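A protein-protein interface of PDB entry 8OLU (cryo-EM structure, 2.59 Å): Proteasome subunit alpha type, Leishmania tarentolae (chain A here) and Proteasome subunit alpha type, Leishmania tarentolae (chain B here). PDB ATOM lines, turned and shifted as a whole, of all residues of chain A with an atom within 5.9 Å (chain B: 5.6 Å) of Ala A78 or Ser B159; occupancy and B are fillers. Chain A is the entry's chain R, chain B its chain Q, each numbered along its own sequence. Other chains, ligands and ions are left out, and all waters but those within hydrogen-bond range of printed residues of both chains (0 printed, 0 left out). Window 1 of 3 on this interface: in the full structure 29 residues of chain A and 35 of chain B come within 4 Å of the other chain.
The side-chain hydroxyl (OG1) of Thr B128 sits at hydrogen-bond distance from the backbone carbonyl oxygen (O) of Gln B125.
The side-chain hydroxyl (OG) of Ser B159 sits at hydrogen-bond distance from the side-chain carboxylate (OD2) of Asp B161 (2.8 Å).
Printed residues of chain A that touch a printed residue of chain B: Ser A77, Ala A78, Asp A79, Arg A81 and Val A82.
Hydrophobic or aromatic side chains of chain A that line the printed part of chain B: Ala A78 and Val A82.
Among the printed residues, no Asp or Glu carboxylate lies within 4 Å of a Lys or Arg side-chain nitrogen of the other chain.
Among the printed residues, merely in contact across the chains: Val A82 with Gln B125, Ser A77 with Asp B161, Ala A78 with Ser B159, Ala A78 with Gln B125 and Ala A78 with Gly B160.
Ala A78 touches four residues of chain B.
Ser B159 touches one residue of chain A.
Of the printed residues of chain A, Cys B121 touches Arg A81 (3.0 Å).
Printed residues of chain A within 4 Å of Gln B125: Ala A78 (3.6 Å), Asp A79 (2.5 Å) and Val A82 (3.4 Å).
Of the printed residues of chain B, Arg A81 touches Cys B121 and Gly B160.
The nearest residue of chain B that does not touch Ala A78 is Cys B121 (5.4 Å).
The nearest printed residue of chain A that does not touch Ser B159 is Asp A79 (5.9 Å).
The backbone carbonyl oxygen of Cys B121 lies within hydrogen-bond range of the guanidinium group of Arg A81, 3.0 Å away.
NE2 of Gln B125 sits at hydrogen-bond distance from OD1 of Asp A79.
NH1 of Arg A81 lies within hydrogen-bond range of O of Gly B160, at 2.9 Å.
The backbone NH (N) of Ala A78 is in hydrogen-bond range of the side-chain carboxylate (OD1) of Asp B161 (3.3 Å).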
ATOM      1  N   GLY A  75       2.699 -21.540   0.158  1.00  0.00           N
ATOM      2  CA  GLY A  75       3.055 -21.449  -1.250  1.00  0.00           C
ATOM      3  C   GLY A  75       2.268 -22.454  -2.051  1.00  0.00           C
ATOM      4  O   GLY A  75       1.166 -22.835  -1.661  1.00  0.00           O
ATOM      5  N   LEU A  76       2.866 -22.996  -3.094  1.00  0.00           N
ATOM      6  CA  LEU A  76       2.123 -23.941  -3.917  1.00  0.00           C
ATOM      7  C   LEU A  76       1.991 -25.272  -3.214  1.00  0.00           C
ATOM      8  O   LEU A  76       2.958 -25.999  -3.040  1.00  0.00           O
ATOM      9  CB  LEU A  76       2.829 -24.083  -5.257  1.00  0.00           C
ATOM     10  CG  LEU A  76       3.081 -22.740  -5.946  1.00  0.00           C
ATOM     11  CD1 LEU A  76       3.712 -22.949  -7.311  1.00  0.00           C
ATOM     12  CD2 LEU A  76       1.797 -21.948  -6.043  1.00  0.00           C
ATOM     13  N   SER A  77       0.737 -25.577  -2.866  1.00  0.00           N
ATOM     14  CA  SER A  77       0.335 -26.857  -2.305  1.00  0.00           C
ATOM     15  C   SER A  77       1.015 -28.058  -2.950  1.00  0.00           C
ATOM     16  O   SER A  77       1.321 -29.019  -2.249  1.00  0.00           O
ATOM     17  CB  SER A  77      -1.129 -27.009  -2.384  1.00  0.00           C
ATOM     18  OG  SER A  77      -1.707 -26.005  -1.581  1.00  0.00           O
ATOM     19  N   ALA A  78       1.124 -28.066  -4.267  1.00  0.00           N
ATOM     20  CA  ALA A  78       1.494 -29.299  -4.922  1.00  0.00           C
ATOM     21  C   ALA A  78       3.011 -29.443  -4.928  1.00  0.00           C
ATOM     22  O   ALA A  78       3.541 -30.568  -4.917  1.00  0.00           O
ATOM     23  CB  ALA A  78       0.974 -29.305  -6.321  1.00  0.00           C
ATOM     24  N   ASP A  79       3.680 -28.295  -5.043  1.00  0.00           N
ATOM     25  CA  ASP A  79       5.104 -28.253  -4.825  1.00  0.00           C
ATOM     26  C   ASP A  79       5.365 -28.722  -3.411  1.00  0.00           C
ATOM     27  O   ASP A  79       6.181 -29.599  -3.181  1.00  0.00           O
ATOM     28  CB  ASP A  79       5.657 -26.856  -5.069  1.00  0.00           C
ATOM     29  CG  ASP A  79       5.671 -26.412  -6.527  1.00  0.00           C
ATOM     30  OD1 ASP A  79       5.215 -27.206  -7.373  1.00  0.00           O
ATOM     31  OD2 ASP A  79       6.131 -25.254  -6.804  1.00  0.00           O
ATOM     32  N   ALA A  80       4.667 -28.144  -2.455  1.00  0.00           N
ATOM     33  CA  ALA A  80       4.891 -28.542  -1.081  1.00  0.00           C
ATOM     34  C   ALA A  80       4.805 -30.045  -0.930  1.00  0.00           C
ATOM     35  O   ALA A  80       5.652 -30.635  -0.268  1.00  0.00           O
ATOM     36  CB  ALA A  80       3.882 -27.910  -0.163  1.00  0.00           C
ATOM     37  N   ARG A  81       3.727 -30.608  -1.471  1.00  0.00           N
ATOM     38  CA  ARG A  81       3.476 -32.026  -1.341  1.00  0.00           C
ATOM     39  C   ARG A  81       4.666 -32.845  -1.841  1.00  0.00           C
ATOM     40  O   ARG A  81       4.994 -33.898  -1.321  1.00  0.00           O
ATOM     41  CB  ARG A  81       2.223 -32.430  -2.101  1.00  0.00           C
ATOM     42  CG  ARG A  81       1.731 -33.815  -1.710  1.00  0.00           C
ATOM     43  CD  ARG A  81       0.560 -34.420  -2.469  1.00  0.00           C
ATOM     44  NE  ARG A  81       0.686 -34.491  -3.938  1.00  0.00           N
ATOM     45  CZ  ARG A  81       0.088 -33.620  -4.768  1.00  0.00           C
ATOM     46  NH1 ARG A  81       0.226 -33.777  -6.083  1.00  0.00           N
ATOM     47  NH2 ARG A  81      -0.605 -32.605  -4.244  1.00  0.00           N
ATOM     48  N   VAL A  82       5.336 -32.349  -2.848  1.00  0.00           N
ATOM     49  CA  VAL A  82       6.478 -33.029  -3.387  1.00  0.00           C
ATOM     50  C   VAL A  82       7.642 -32.909  -2.440  1.00  0.00           C
ATOM     51  O   VAL A  82       8.258 -33.897  -2.061  1.00  0.00           O
ATOM     52  CB  VAL A  82       6.814 -32.462  -4.760  1.00  0.00           C
ATOM     53  CG1 VAL A  82       8.189 -32.855  -5.216  1.00  0.00           C
ATOM     54  CG2 VAL A  82       5.813 -32.959  -5.756  1.00  0.00           C
ATOM     55  N   LEU A  83       7.962 -31.712  -2.035  1.00  0.00           N
ATOM     56  CA  LEU A  83       8.976 -31.560  -1.019  1.00  0.00           C
ATOM     57  C   LEU A  83       8.794 -32.469   0.169  1.00  0.00           C
ATOM     58  O   LEU A  83       9.734 -33.005   0.684  1.00  0.00           O
ATOM     59  CB  LEU A  83       8.856 -30.151  -0.515  1.00  0.00           C
ATOM     60  CG  LEU A  83      10.146 -29.385  -0.595  1.00  0.00           C
ATOM     61  CD1 LEU A  83      10.838 -29.662  -1.909  1.00  0.00           C
ATOM     62  CD2 LEU A  83       9.813 -27.922  -0.427  1.00  0.00           C
ATOM     63  N   VAL B  21      -0.591 -23.122 -16.006  1.00  0.00           N
ATOM     64  CA  VAL B  21      -1.554 -23.791 -15.128  1.00  0.00           C
ATOM     65  C   VAL B  21      -2.795 -22.934 -14.987  1.00  0.00           C
ATOM     66  O   VAL B  21      -3.883 -23.470 -14.990  1.00  0.00           O
ATOM     67  CB  VAL B  21      -0.954 -24.114 -13.761  1.00  0.00           C
ATOM     68  CG1 VAL B  21      -1.955 -24.654 -12.797  1.00  0.00           C
ATOM     69  CG2 VAL B  21       0.176 -25.129 -13.888  1.00  0.00           C
ATOM     70  N   CYS B 121      -2.025 -36.682  -9.065  1.00  0.00           N
ATOM     71  CA  CYS B 121      -1.649 -35.303  -8.962  1.00  0.00           C
ATOM     72  C   CYS B 121      -0.150 -35.078  -8.869  1.00  0.00           C
ATOM     73  O   CYS B 121       0.319 -33.966  -9.045  1.00  0.00           O
ATOM     74  CB  CYS B 121      -2.319 -34.796  -7.710  1.00  0.00           C
ATOM     75  SG  CYS B 121      -4.114 -34.884  -7.938  1.00  0.00           S
ATOM     76  N   LYS B 124       0.587 -34.905 -12.502  1.00  0.00           N
ATOM     77  CA  LYS B 124       0.376 -33.551 -12.940  1.00  0.00           C
ATOM     78  C   LYS B 124       1.360 -32.539 -12.384  1.00  0.00           C
ATOM     79  O   LYS B 124       1.775 -31.648 -13.079  1.00  0.00           O
ATOM     80  CB  LYS B 124      -1.016 -33.163 -12.489  1.00  0.00           C
ATOM     81  CG  LYS B 124      -2.012 -34.105 -13.134  1.00  0.00           C
ATOM     82  CD  LYS B 124      -3.313 -33.438 -13.401  1.00  0.00           C
ATOM     83  CE  LYS B 124      -4.261 -33.604 -12.251  1.00  0.00           C
ATOM     84  NZ  LYS B 124      -5.597 -33.214 -12.731  1.00  0.00           N
ATOM     85  N   GLN B 125       1.637 -32.529 -11.117  1.00  0.00           N
ATOM     86  CA  GLN B 125       2.544 -31.515 -10.640  1.00  0.00           C
ATOM     87  C   GLN B 125       3.825 -31.535 -11.472  1.00  0.00           C
ATOM     88  O   GLN B 125       4.380 -30.471 -11.695  1.00  0.00           O
ATOM     89  CB  GLN B 125       2.864 -31.736  -9.161  1.00  0.00           C
ATOM     90  CG  GLN B 125       3.591 -30.592  -8.495  1.00  0.00           C
ATOM     91  CD  GLN B 125       5.083 -30.596  -8.609  1.00  0.00           C
ATOM     92  OE1 GLN B 125       5.727 -31.599  -8.894  1.00  0.00           O
ATOM     93  NE2 GLN B 125       5.642 -29.438  -8.361  1.00  0.00           N
ATOM     94  N   THR B 128       4.296 -29.172 -14.255  1.00  0.00           N
ATOM     95  CA  THR B 128       4.286 -27.763 -13.944  1.00  0.00           C
ATOM     96  C   THR B 128       5.632 -27.307 -13.442  1.00  0.00           C
ATOM     97  O   THR B 128       5.765 -26.141 -13.111  1.00  0.00           O
ATOM     98  CB  THR B 128       3.225 -27.463 -12.912  1.00  0.00           C
ATOM     99  OG1 THR B 128       3.561 -28.061 -11.656  1.00  0.00           O
ATOM    100  CG2 THR B 128       1.900 -27.988 -13.403  1.00  0.00           C
ATOM    101  N   GLU B 157      -6.801 -30.695  -9.797  1.00  0.00           N
ATOM    102  CA  GLU B 157      -6.634 -29.562 -10.660  1.00  0.00           C
ATOM    103  C   GLU B 157      -5.383 -29.788 -11.491  1.00  0.00           C
ATOM    104  O   GLU B 157      -4.524 -30.618 -11.194  1.00  0.00           O
ATOM    105  CB  GLU B 157      -6.463 -28.309  -9.819  1.00  0.00           C
ATOM    106  CG  GLU B 157      -7.674 -28.047  -8.957  1.00  0.00           C
ATOM    107  CD  GLU B 157      -7.713 -26.693  -8.258  1.00  0.00           C
ATOM    108  OE1 GLU B 157      -6.851 -25.822  -8.558  1.00  0.00           O
ATOM    109  OE2 GLU B 157      -8.609 -26.514  -7.397  1.00  0.00           O
ATOM    110  N   PRO B 158      -5.173 -28.996 -12.535  1.00  0.00           N
ATOM    111  CA  PRO B 158      -3.957 -29.158 -13.305  1.00  0.00           C
ATOM    112  C   PRO B 158      -2.665 -28.808 -12.581  1.00  0.00           C
ATOM    113  O   PRO B 158      -1.610 -29.234 -13.049  1.00  0.00           O
ATOM    114  CB  PRO B 158      -4.175 -28.168 -14.429  1.00  0.00           C
ATOM    115  CG  PRO B 158      -5.649 -27.970 -14.450  1.00  0.00           C
ATOM    116  CD  PRO B 158      -6.022 -27.896 -12.989  1.00  0.00           C
ATOM    117  N   SER B 159      -2.722 -28.010 -11.503  1.00  0.00           N
ATOM    118  CA  SER B 159      -1.530 -27.699 -10.722  1.00  0.00           C
ATOM    119  C   SER B 159      -0.990 -28.948 -10.046  1.00  0.00           C
ATOM    120  O   SER B 159       0.207 -29.044  -9.783  1.00  0.00           O
ATOM    121  CB  SER B 159      -1.792 -26.652  -9.693  1.00  0.00           C
ATOM    122  OG  SER B 159      -3.160 -26.652  -9.351  1.00  0.00           O
ATOM    123  N   GLY B 160      -1.892 -29.888  -9.750  1.00  0.00           N
ATOM    124  CA  GLY B 160      -1.549 -31.096  -9.017  1.00  0.00           C
ATOM    125  C   GLY B 160      -2.076 -31.020  -7.594  1.00  0.00           C
ATOM    126  O   GLY B 160      -1.791 -31.893  -6.805  1.00  0.00           O
ATOM    127  N   ASP B 161      -2.800 -29.955  -7.247  1.00  0.00           N
ATOM    128  CA  ASP B 161      -3.400 -29.923  -5.927  1.00  0.00           C
ATOM    129  C   ASP B 161      -4.643 -30.786  -5.995  1.00  0.00           C
ATOM    130  O   ASP B 161      -5.145 -31.075  -7.057  1.00  0.00           O
ATOM    131  CB  ASP B 161      -3.809 -28.541  -5.415  1.00  0.00           C
ATOM    132  CG  ASP B 161      -2.975 -27.381  -5.939  1.00  0.00           C
ATOM    133  OD1 ASP B 161      -1.712 -27.390  -5.746  1.00  0.00           O
ATOM    134  OD2 ASP B 161      -3.590 -26.453  -6.542  1.00  0.00           O
